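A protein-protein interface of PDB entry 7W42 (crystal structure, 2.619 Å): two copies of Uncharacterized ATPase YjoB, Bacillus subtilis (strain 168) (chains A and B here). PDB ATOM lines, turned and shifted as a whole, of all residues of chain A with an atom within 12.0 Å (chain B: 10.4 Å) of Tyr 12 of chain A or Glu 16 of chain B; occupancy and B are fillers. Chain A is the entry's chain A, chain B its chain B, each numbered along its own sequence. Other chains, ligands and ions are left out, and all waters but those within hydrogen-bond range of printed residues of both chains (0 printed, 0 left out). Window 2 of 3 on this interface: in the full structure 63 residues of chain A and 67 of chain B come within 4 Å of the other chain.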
ATOM      1  N   PRO A   7      12.435 -12.703 -16.866  1.00  0.00           N
ATOM      2  CA  PRO A   7      12.157 -13.720 -15.834  1.00  0.00           C
ATOM      3  C   PRO A   7      10.993 -13.297 -14.945  1.00  0.00           C
ATOM      4  O   PRO A   7      10.636 -12.108 -14.859  1.00  0.00           O
ATOM      5  CB  PRO A   7      13.459 -13.812 -15.018  1.00  0.00           C
ATOM      6  CG  PRO A   7      14.454 -12.900 -15.697  1.00  0.00           C
ATOM      7  CD  PRO A   7      13.676 -11.954 -16.557  1.00  0.00           C
ATOM      8  N   PHE A   8      10.409 -14.299 -14.266  1.00  0.00           N
ATOM      9  CA  PHE A   8       9.372 -14.067 -13.264  1.00  0.00           C
ATOM     10  C   PHE A   8       9.827 -14.590 -11.907  1.00  0.00           C
ATOM     11  O   PHE A   8      10.187 -15.762 -11.765  1.00  0.00           O
ATOM     12  CB  PHE A   8       8.032 -14.677 -13.690  1.00  0.00           C
ATOM     13  CG  PHE A   8       7.429 -13.996 -14.892  1.00  0.00           C
ATOM     14  CD1 PHE A   8       7.144 -12.645 -14.858  1.00  0.00           C
ATOM     15  CD2 PHE A   8       7.205 -14.687 -16.068  1.00  0.00           C
ATOM     16  CE1 PHE A   8       6.624 -11.998 -15.964  1.00  0.00           C
ATOM     17  CE2 PHE A   8       6.687 -14.047 -17.178  1.00  0.00           C
ATOM     18  CZ  PHE A   8       6.396 -12.698 -17.120  1.00  0.00           C
ATOM     19  N   ILE A   9       9.831 -13.695 -10.919  1.00  0.00           N
ATOM     20  CA  ILE A   9      10.210 -14.056  -9.558  1.00  0.00           C
ATOM     21  C   ILE A   9       9.263 -15.111  -9.003  1.00  0.00           C
ATOM     22  O   ILE A   9       9.690 -16.156  -8.500  1.00  0.00           O
ATOM     23  CB  ILE A   9      10.243 -12.792  -8.672  1.00  0.00           C
ATOM     24  CG1 ILE A   9      11.308 -11.810  -9.189  1.00  0.00           C
ATOM     25  CG2 ILE A   9      10.432 -13.153  -7.188  1.00  0.00           C
ATOM     26  CD1 ILE A   9      12.651 -12.481  -9.595  1.00  0.00           C
ATOM     27  N   TYR A  10       7.965 -14.846  -9.079  1.00  0.00           N
ATOM     28  CA  TYR A  10       6.948 -15.738  -8.542  1.00  0.00           C
ATOM     29  C   TYR A  10       6.653 -16.831  -9.549  1.00  0.00           C
ATOM     30  O   TYR A  10       6.160 -16.556 -10.649  1.00  0.00           O
ATOM     31  CB  TYR A  10       5.684 -14.953  -8.244  1.00  0.00           C
ATOM     32  CG  TYR A  10       4.597 -15.651  -7.459  1.00  0.00           C
ATOM     33  CD1 TYR A  10       4.689 -15.791  -6.077  1.00  0.00           C
ATOM     34  CD2 TYR A  10       3.435 -16.089  -8.091  1.00  0.00           C
ATOM     35  CE1 TYR A  10       3.668 -16.366  -5.350  1.00  0.00           C
ATOM     36  CE2 TYR A  10       2.408 -16.665  -7.377  1.00  0.00           C
ATOM     37  CZ  TYR A  10       2.524 -16.803  -6.005  1.00  0.00           C
ATOM     38  OH  TYR A  10       1.489 -17.382  -5.296  1.00  0.00           O
ATOM     39  N   GLN A  11       6.954 -18.068  -9.170  1.00  0.00           N
ATOM     40  CA  GLN A  11       6.785 -19.207 -10.046  1.00  0.00           C
ATOM     41  C   GLN A  11       5.807 -20.219  -9.479  1.00  0.00           C
ATOM     42  O   GLN A  11       5.626 -21.284 -10.073  1.00  0.00           O
ATOM     43  CB  GLN A  11       8.141 -19.863 -10.308  1.00  0.00           C
ATOM     44  CG  GLN A  11       9.154 -18.969 -11.016  1.00  0.00           C
ATOM     45  CD  GLN A  11      10.420 -19.745 -11.390  1.00  0.00           C
ATOM     46  OE1 GLN A  11      10.725 -19.933 -12.578  1.00  0.00           O
ATOM     47  NE2 GLN A  11      11.157 -20.210 -10.372  1.00  0.00           N
ATOM     48  N   TYR A  12       5.182 -19.917  -8.348  1.00  0.00           N
ATOM     49  CA  TYR A  12       4.204 -20.808  -7.744  1.00  0.00           C
ATOM     50  C   TYR A  12       3.037 -21.030  -8.695  1.00  0.00           C
ATOM     51  O   TYR A  12       2.566 -20.098  -9.355  1.00  0.00           O
ATOM     52  CB  TYR A  12       3.704 -20.200  -6.438  1.00  0.00           C
ATOM     53  CG  TYR A  12       2.619 -21.002  -5.766  1.00  0.00           C
ATOM     54  CD1 TYR A  12       2.933 -22.130  -5.016  1.00  0.00           C
ATOM     55  CD2 TYR A  12       1.278 -20.639  -5.876  1.00  0.00           C
ATOM     56  CE1 TYR A  12       1.952 -22.869  -4.390  1.00  0.00           C
ATOM     57  CE2 TYR A  12       0.284 -21.378  -5.254  1.00  0.00           C
ATOM     58  CZ  TYR A  12       0.634 -22.488  -4.510  1.00  0.00           C
ATOM     59  OH  TYR A  12      -0.328 -23.236  -3.880  1.00  0.00           O
ATOM     60  N   GLU A  13       2.558 -22.268  -8.776  1.00  0.00           N
ATOM     61  CA  GLU A  13       1.449 -22.561  -9.672  1.00  0.00           C
ATOM     62  C   GLU A  13       0.182 -22.839  -8.880  1.00  0.00           C
ATOM     63  O   GLU A  13       0.160 -23.709  -8.000  1.00  0.00           O
ATOM     64  CB  GLU A  13       1.767 -23.696 -10.642  1.00  0.00           C
ATOM     65  CG  GLU A  13       2.267 -23.149 -11.995  1.00  0.00           C
ATOM     66  CD  GLU A  13       1.475 -21.914 -12.509  1.00  0.00           C
ATOM     67  OE1 GLU A  13       2.064 -21.110 -13.280  1.00  0.00           O
ATOM     68  OE2 GLU A  13       0.270 -21.751 -12.177  1.00  0.00           O
ATOM     69  N   GLU A  14      -0.860 -22.081  -9.209  1.00  0.00           N
ATOM     70  CA  GLU A  14      -2.101 -22.044  -8.453  1.00  0.00           C
ATOM     71  C   GLU A  14      -2.958 -23.263  -8.777  1.00  0.00           C
ATOM     72  O   GLU A  14      -3.232 -23.543  -9.950  1.00  0.00           O
ATOM     73  CB  GLU A  14      -2.871 -20.756  -8.793  1.00  0.00           C
ATOM     74  CG  GLU A  14      -2.705 -19.557  -7.827  1.00  0.00           C
ATOM     75  CD  GLU A  14      -1.656 -18.498  -8.259  1.00  0.00           C
ATOM     76  OE1 GLU A  14      -1.364 -18.358  -9.479  1.00  0.00           O
ATOM     77  OE2 GLU A  14      -1.115 -17.811  -7.347  1.00  0.00           O
ATOM     78  N   LYS A  15      -3.376 -23.990  -7.737  1.00  0.00           N
ATOM     79  CA  LYS A  15      -4.508 -24.897  -7.886  1.00  0.00           C
ATOM     80  C   LYS A  15      -5.703 -24.113  -8.413  1.00  0.00           C
ATOM     81  O   LYS A  15      -5.857 -22.922  -8.134  1.00  0.00           O
ATOM     82  CB  LYS A  15      -4.874 -25.556  -6.551  1.00  0.00           C
ATOM     83  CG  LYS A  15      -3.724 -26.195  -5.802  1.00  0.00           C
ATOM     84  CD  LYS A  15      -3.470 -27.617  -6.278  1.00  0.00           C
ATOM     85  CE  LYS A  15      -2.500 -28.340  -5.350  1.00  0.00           C
ATOM     86  NZ  LYS A  15      -2.213 -29.747  -5.784  1.00  0.00           N
ATOM     87  N   GLU A  16      -6.556 -24.776  -9.192  1.00  0.00           N
ATOM     88  CA  GLU A  16      -7.721 -24.067  -9.701  1.00  0.00           C
ATOM     89  C   GLU A  16      -8.670 -23.666  -8.569  1.00  0.00           C
ATOM     90  O   GLU A  16      -9.447 -22.718  -8.732  1.00  0.00           O
ATOM     91  CB  GLU A  16      -8.411 -24.910 -10.782  1.00  0.00           C
ATOM     92  CG  GLU A  16      -7.388 -25.716 -11.645  1.00  0.00           C
ATOM     93  CD  GLU A  16      -7.690 -25.739 -13.160  1.00  0.00           C
ATOM     94  OE1 GLU A  16      -8.883 -25.772 -13.548  1.00  0.00           O
ATOM     95  OE2 GLU A  16      -6.719 -25.735 -13.960  1.00  0.00           O
ATOM     96  N   ASN A  17      -8.578 -24.322  -7.404  1.00  0.00           N
ATOM     97  CA  ASN A  17      -9.361 -23.924  -6.242  1.00  0.00           C
ATOM     98  C   ASN A  17      -8.948 -22.555  -5.698  1.00  0.00           C
ATOM     99  O   ASN A  17      -9.749 -21.899  -5.017  1.00  0.00           O
ATOM    100  CB  ASN A  17      -9.238 -24.980  -5.134  1.00  0.00           C
ATOM    101  CG  ASN A  17     -10.444 -25.934  -5.076  1.00  0.00           C
ATOM    102  OD1 ASN A  17     -11.173 -26.109  -6.062  1.00  0.00           O
ATOM    103  ND2 ASN A  17     -10.652 -26.553  -3.910  1.00  0.00           N
ATOM    104  N   GLU A  18      -7.723 -22.112  -5.969  1.00  0.00           N
ATOM    105  CA  GLU A  18      -7.235 -20.815  -5.523  1.00  0.00           C
ATOM    106  C   GLU A  18      -7.623 -19.681  -6.454  1.00  0.00           C
ATOM    107  O   GLU A  18      -7.237 -18.534  -6.203  1.00  0.00           O
ATOM    108  CB  GLU A  18      -5.704 -20.827  -5.400  1.00  0.00           C
ATOM    109  CG  GLU A  18      -5.135 -22.018  -4.658  1.00  0.00           C
ATOM    110  CD  GLU A  18      -3.616 -22.045  -4.682  1.00  0.00           C
ATOM    111  OE1 GLU A  18      -3.011 -21.209  -5.394  1.00  0.00           O
ATOM    112  OE2 GLU A  18      -3.034 -22.918  -4.005  1.00  0.00           O
ATOM    113  N   ARG A  19      -8.325 -19.963  -7.547  1.00  0.00           N
ATOM    114  CA  ARG A  19      -8.811 -18.882  -8.394  1.00  0.00           C
ATOM    115  C   ARG A  19     -10.081 -18.251  -7.834  1.00  0.00           C
ATOM    116  O   ARG A  19     -10.435 -17.139  -8.250  1.00  0.00           O
ATOM    117  CB  ARG A  19      -9.004 -19.406  -9.825  1.00  0.00           C
ATOM    118  CG  ARG A  19      -7.802 -20.279 -10.239  1.00  0.00           C
ATOM    119  CD  ARG A  19      -7.623 -20.485 -11.735  1.00  0.00           C
ATOM    120  NE  ARG A  19      -8.825 -21.008 -12.368  1.00  0.00           N
ATOM    121  CZ  ARG A  19      -8.842 -21.570 -13.573  1.00  0.00           C
ATOM    122  NH1 ARG A  19      -7.713 -21.679 -14.271  1.00  0.00           N
ATOM    123  NH2 ARG A  19      -9.990 -22.025 -14.079  1.00  0.00           N
ATOM    124  N   ALA A  20     -10.709 -18.896  -6.842  1.00  0.00           N
ATOM    125  CA  ALA A  20     -12.024 -18.496  -6.359  1.00  0.00           C
ATOM    126  C   ALA A  20     -12.020 -17.082  -5.798  1.00  0.00           C
ATOM    127  O   ALA A  20     -11.070 -16.658  -5.134  1.00  0.00           O
ATOM    128  CB  ALA A  20     -12.508 -19.469  -5.286  1.00  0.00           C
ATOM    129  N   TYR B  12      11.545 -23.282  11.172  1.00  0.00           N
ATOM    130  CA  TYR B  12      10.493 -23.943  10.406  1.00  0.00           C
ATOM    131  C   TYR B  12      10.757 -23.785   8.917  1.00  0.00           C
ATOM    132  O   TYR B  12      11.132 -22.708   8.451  1.00  0.00           O
ATOM    133  CB  TYR B  12       9.139 -23.333  10.766  1.00  0.00           C
ATOM    134  CG  TYR B  12       7.946 -23.896  10.045  1.00  0.00           C
ATOM    135  CD1 TYR B  12       7.387 -25.102  10.435  1.00  0.00           C
ATOM    136  CD2 TYR B  12       7.343 -23.203   9.002  1.00  0.00           C
ATOM    137  CE1 TYR B  12       6.272 -25.622   9.786  1.00  0.00           C
ATOM    138  CE2 TYR B  12       6.223 -23.710   8.343  1.00  0.00           C
ATOM    139  CZ  TYR B  12       5.691 -24.919   8.745  1.00  0.00           C
ATOM    140  OH  TYR B  12       4.580 -25.443   8.115  1.00  0.00           O
ATOM    141  N   GLU B  13      10.584 -24.859   8.158  1.00  0.00           N
ATOM    142  CA  GLU B  13      10.664 -24.760   6.705  1.00  0.00           C
ATOM    143  C   GLU B  13       9.266 -24.853   6.115  1.00  0.00           C
ATOM    144  O   GLU B  13       8.395 -25.545   6.655  1.00  0.00           O
ATOM    145  CB  GLU B  13      11.568 -25.823   6.095  1.00  0.00           C
ATOM    146  CG  GLU B  13      11.759 -25.620   4.581  1.00  0.00           C
ATOM    147  CD  GLU B  13      11.857 -26.925   3.786  1.00  0.00           C
ATOM    148  OE1 GLU B  13      11.339 -26.954   2.643  1.00  0.00           O
ATOM    149  OE2 GLU B  13      12.466 -27.906   4.283  1.00  0.00           O
ATOM    150  N   GLU B  14       9.057 -24.151   5.011  1.00  0.00           N
ATOM    151  CA  GLU B  14       7.731 -23.911   4.463  1.00  0.00           C
ATOM    152  C   GLU B  14       7.404 -24.943   3.387  1.00  0.00           C
ATOM    153  O   GLU B  14       8.232 -25.222   2.510  1.00  0.00           O
ATOM    154  CB  GLU B  14       7.658 -22.484   3.905  1.00  0.00           C
ATOM    155  CG  GLU B  14       7.874 -21.403   4.973  1.00  0.00           C
ATOM    156  CD  GLU B  14       9.270 -20.741   4.938  1.00  0.00           C
ATOM    157  OE1 GLU B  14       9.459 -19.793   4.132  1.00  0.00           O
ATOM    158  OE2 GLU B  14      10.168 -21.149   5.721  1.00  0.00           O
ATOM    159  N   LYS B  15       6.208 -25.524   3.472  1.00  0.00           N
ATOM    160  CA  LYS B  15       5.714 -26.323   2.361  1.00  0.00           C
ATOM    161  C   LYS B  15       5.425 -25.415   1.167  1.00  0.00           C
ATOM    162  O   LYS B  15       5.261 -24.200   1.300  1.00  0.00           O
ATOM    163  CB  LYS B  15       4.464 -27.107   2.761  1.00  0.00           C
ATOM    164  CG  LYS B  15       4.350 -27.479   4.248  1.00  0.00           C
ATOM    165  CD  LYS B  15       5.531 -28.316   4.769  1.00  0.00           C
ATOM    166  CE  LYS B  15       5.954 -27.830   6.157  1.00  0.00           C
ATOM    167  NZ  LYS B  15       4.788 -27.738   7.091  1.00  0.00           N
ATOM    168  N   GLU B  16       5.367 -26.019  -0.021  1.00  0.00           N
ATOM    169  CA  GLU B  16       5.360 -25.207  -1.232  1.00  0.00           C
ATOM    170  C   GLU B  16       4.087 -24.382  -1.380  1.00  0.00           C
ATOM    171  O   GLU B  16       4.118 -23.337  -2.034  1.00  0.00           O
ATOM    172  CB  GLU B  16       5.560 -26.081  -2.463  1.00  0.00           C
ATOM    173  CG  GLU B  16       6.237 -25.344  -3.612  1.00  0.00           C
ATOM    174  CD  GLU B  16       5.711 -25.766  -4.979  1.00  0.00           C
ATOM    175  OE1 GLU B  16       5.935 -25.003  -5.958  1.00  0.00           O
ATOM    176  OE2 GLU B  16       5.084 -26.855  -5.071  1.00  0.00           O
ATOM    177  N   ASN B  17       2.963 -24.803  -0.800  1.00  0.00           N
ATOM    178  CA  ASN B  17       1.751 -24.013  -0.998  1.00  0.00           C
ATOM    179  C   ASN B  17       1.617 -22.878   0.012  1.00  0.00           C
ATOM    180  O   ASN B  17       0.690 -22.070  -0.097  1.00  0.00           O
ATOM    181  CB  ASN B  17       0.496 -24.912  -1.013  1.00  0.00           C
ATOM    182  CG  ASN B  17       0.091 -25.419   0.367  1.00  0.00           C
ATOM    183  OD1 ASN B  17       0.910 -25.508   1.286  1.00  0.00           O
ATOM    184  ND2 ASN B  17      -1.188 -25.780   0.505  1.00  0.00           N
ATOM    185  N   GLU B  18       2.546 -22.769   0.957  1.00  0.00           N
ATOM    186  CA  GLU B  18       2.621 -21.589   1.803  1.00  0.00           C
ATOM    187  C   GLU B  18       3.240 -20.384   1.099  1.00  0.00           C
ATOM    188  O   GLU B  18       3.228 -19.286   1.664  1.00  0.00           O
ATOM    189  CB  GLU B  18       3.436 -21.887   3.061  1.00  0.00           C
ATOM    190  CG  GLU B  18       2.813 -22.881   4.017  1.00  0.00           C
ATOM    191  CD  GLU B  18       3.558 -22.923   5.338  1.00  0.00           C
ATOM    192  OE1 GLU B  18       3.167 -23.732   6.207  1.00  0.00           O
ATOM    193  OE2 GLU B  18       4.538 -22.145   5.498  1.00  0.00           O
ATOM    194  N   ARG B  19       3.800 -20.543  -0.097  1.00  0.00           N
ATOM    195  CA  ARG B  19       4.316 -19.372  -0.785  1.00  0.00           C
ATOM    196  C   ARG B  19       3.243 -18.657  -1.602  1.00  0.00           C
ATOM    197  O   ARG B  19       3.507 -17.573  -2.140  1.00  0.00           O
ATOM    198  CB  ARG B  19       5.531 -19.748  -1.650  1.00  0.00           C
ATOM    199  CG  ARG B  19       5.290 -20.584  -2.885  1.00  0.00           C
ATOM    200  CD  ARG B  19       6.570 -21.332  -3.314  1.00  0.00           C
ATOM    201  NE  ARG B  19       7.454 -21.657  -2.183  1.00  0.00           N
ATOM    202  CZ  ARG B  19       8.542 -22.427  -2.269  1.00  0.00           C
ATOM    203  NH1 ARG B  19       8.883 -22.968  -3.441  1.00  0.00           N
ATOM    204  NH2 ARG B  19       9.295 -22.648  -1.184  1.00  0.00           N
ATOM    205  N   ALA B  20       2.031 -19.201  -1.661  1.00  0.00           N
ATOM    206  CA  ALA B  20       0.969 -18.568  -2.431  1.00  0.00           C
ATOM    207  C   ALA B  20       0.678 -17.170  -1.904  1.00  0.00           C
ATOM    208  O   ALA B  20       0.574 -16.955  -0.693  1.00  0.00           O
ATOM    209  CB  ALA B  20      -0.301 -19.414  -2.383  1.00  0.00           C
ATOM    210  N   ALA B  21       0.538 -16.220  -2.826  1.00  0.00           N
ATOM    211  CA  ALA B  21       0.293 -14.828  -2.475  1.00  0.00           C
ATOM    212  C   ALA B  21      -1.205 -14.531  -2.428  1.00  0.00           C
ATOM    213  O   ALA B  21      -1.933 -14.788  -3.392  1.00  0.00           O
ATOM    214  CB  ALA B  21       0.997 -13.900  -3.465  1.00  0.00           C
ATOM    215  N   ALA B  22      -1.644 -13.963  -1.307  1.00  0.00           N
ATOM    216  CA  ALA B  22      -3.052 -13.679  -1.063  1.00  0.00           C
ATOM    217  C   ALA B  22      -3.675 -12.829  -2.166  1.00  0.00           C
ATOM    218  O   ALA B  22      -3.179 -11.746  -2.497  1.00  0.00           O
ATOM    219  CB  ALA B  22      -3.203 -12.959   0.275  1.00  0.00           C
ATOM    220  N   GLY B  23      -4.797 -13.303  -2.708  1.00  0.00           N
ATOM    221  CA  GLY B  23      -5.553 -12.540  -3.673  1.00  0.00           C
ATOM    222  C   GLY B  23      -5.017 -12.580  -5.080  1.00  0.00           C
ATOM    223  O   GLY B  23      -5.760 -12.245  -6.010  1.00  0.00           O
ATOM    224  N   TYR B  24      -3.760 -13.014  -5.276  1.00  0.00           N
ATOM    225  CA  TYR B  24      -3.185 -13.054  -6.621  1.00  0.00           C
ATOM    226  C   TYR B  24      -3.801 -14.156  -7.468  1.00  0.00           C
ATOM    227  O   TYR B  24      -3.888 -14.012  -8.691  1.00  0.00           O
ATOM    228  CB  TYR B  24      -1.664 -13.243  -6.571  1.00  0.00           C
ATOM    229  CG  TYR B  24      -1.060 -13.379  -7.950  1.00  0.00           C
ATOM    230  CD1 TYR B  24      -1.075 -12.312  -8.848  1.00  0.00           C
ATOM    231  CD2 TYR B  24      -0.502 -14.576  -8.369  1.00  0.00           C
ATOM    232  CE1 TYR B  24      -0.545 -12.433 -10.134  1.00  0.00           C
ATOM    233  CE2 TYR B  24       0.036 -14.712  -9.646  1.00  0.00           C
ATOM    234  CZ  TYR B  24       0.013 -13.640 -10.533  1.00  0.00           C
ATOM    235  OH  TYR B  24       0.556 -13.789 -11.810  1.00  0.00           O
ATOM    236  N   GLY B  25      -4.228 -15.256  -6.842  1.00  0.00           N
ATOM    237  CA  GLY B  25      -4.842 -16.341  -7.594  1.00  0.00           C
ATOM    238  C   GLY B  25      -6.084 -15.901  -8.342  1.00  0.00           C
ATOM    239  O   GLY B  25      -6.231 -16.172  -9.534  1.00  0.00           O
ATOM    240  N   THR B  26      -6.983 -15.191  -7.656  1.00  0.00           N
ATOM    241  CA  THR B  26      -8.155 -14.628  -8.324  1.00  0.00           C
ATOM    242  C   THR B  26      -7.749 -13.558  -9.335  1.00  0.00           C
ATOM    243  O   THR B  26      -8.181 -13.578 -10.496  1.00  0.00           O
ATOM    244  CB  THR B  26      -9.122 -14.033  -7.290  1.00  0.00           C
ATOM    245  OG1 THR B  26      -9.423 -15.002  -6.275  1.00  0.00           O
ATOM    246  CG2 THR B  26     -10.422 -13.549  -7.951  1.00  0.00           C
ATOM    247  N   GLY B  28      -4.873 -12.749 -10.952  1.00  0.00           N
ATOM    248  CA  GLY B  28      -4.134 -13.129 -12.144  1.00  0.00           C
ATOM    249  C   GLY B  28      -4.957 -13.960 -13.107  1.00  0.00           C
ATOM    250  O   GLY B  28      -4.786 -13.863 -14.327  1.00  0.00           O
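The side-chain hydroxyl of Tyr 10 of chain A lies within hydrogen-bond range of the backbone NH of Ala 21 of chain B.
O of Arg 19 of chain A lies within hydrogen-bond range of OG1 of Thr 26 of chain B.
OG1 of Thr 26 of chain B lies within hydrogen-bond range of O of Ala 20 of chain A.
OE2 of Glu 14 of chain A sits at hydrogen-bond distance from OH of Tyr 10 of chain A, at 3.3 Å.
The side-chain hydroxyl (OH) of Tyr 12 of chain A sits at hydrogen-bond distance from the side-chain carboxylate (OE2) of Glu 18 of chain A (2.7 Å).
The side-chain carboxylate (OE1) of Glu 16 of chain A is in salt-bridge range of the guanidinium group (NH2) of Arg 19 of chain A (3.9 Å).
Among the printed residues, merely in contact across the chains: Tyr 10 of chain A with Arg 19 of chain B, Tyr 10 of chain A with Ala 20 of chain B, Tyr 10 of chain A with Tyr 24 of chain B, Tyr 12 of chain A with Glu 16 of chain B, Tyr 12 of chain A with Asn 17 of chain B, Tyr 12 of chain A with Arg 19 of chain B, Tyr 12 of chain A with Ala 20 of chain B, Glu 14 of chain A with Tyr 24 of chain B, Glu 14 of chain A with Gly 25 of chain B, Glu 18 of chain A with Gly 25 of chain B, Glu 18 of chain A with Thr 26 of chain B and Arg 19 of chain A with Gly 25 of chain B.
Of chain B, only Arg 19, Ala 20, Ala 21 and Tyr 24 come within 4 Å of Tyr 10 of chain A.
Printed residues of chain B within 4 Å of Glu 14 of chain A: Tyr 24 (3.4 Å) and Gly 25 (3.9 Å).
Asn 17 of chain A touches none of the printed residues of chain B.
Of the printed residues of chain B, Glu 18 of chain A touches Gly 25 and Thr 26.
Of the printed residues of chain B, Arg 19 of chain A touches Gly 25 and Thr 26.
Printed residues of chain B within 4 Å of Ala 20 of chain A: Thr 26.
Tyr 12 of chain B touches none of the printed residues of chain A.
No residue of chain A comes within 4 Å of Lys 15 of chain B.
Of chain A, only Tyr 12 comes within 4 Å of Glu 16 of chain B.
No residue of chain A comes within 4 Å of Glu 18 of chain B.
Ala 20 of chain B touches just these residues of chain A: Tyr 10 (3.1 Å) and Tyr 12 (3.5 Å).
Of the printed residues of chain A, Tyr 24 of chain B touches Tyr 10 (3.7 Å) and Glu 14 (3.4 Å).
Printed residues of chain A within 4 Å of Thr 26 of chain B: Glu 18, Arg 19 and Ala 20.
The nearest residue of chain B that does not touch Tyr 12 of chain A is Glu 18 of chain B (5.4 Å).
The nearest printed residue of chain B that does not touch Glu 18 of chain A is Ala 20 of chain B (4.4 Å).
Of the 16 printed residues of chain B, 8 touch a printed residue of chain A.
Hydrophobic or aromatic side chains of chain B within 4 Å of the printed part of chain A: Ala 20, Ala 21 and Tyr 24.
Hydrophobic or aromatic side chains of chain A that line the printed part of chain B: Tyr 10 and Tyr 12.
Among the printed residues, 15 pairs touch across the chains.
Among the printed residues, no Asp or Glu carboxylate lies within 4 Å of a Lys or Arg side-chain nitrogen of the other chain.
Tyr 12 of chain A touches Glu 16 of chain B, but with the chains exchanged Glu 16 of chain A does not touch Tyr 12 of chain B (20.6 Å).
Tyr 12 of chain A touches Asn 17 of chain B, but with the chains exchanged Asn 17 of chain A does not touch Tyr 12 of chain B (19.1 Å).
Tyr 12 of chain A touches Arg 19 of chain B, but with the chains exchanged Arg 19 of chain A does not touch Tyr 12 of chain B (21.0 Å).
Tyr 12 of chain A touches Ala 20 of chain B, but with the chains exchanged Ala 20 of chain A does not touch Tyr 12 of chain B (22.3 Å).
Of the 15 pairs that touch across the chains among the printed residues, none has its exchanged pair printed and touching as well.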
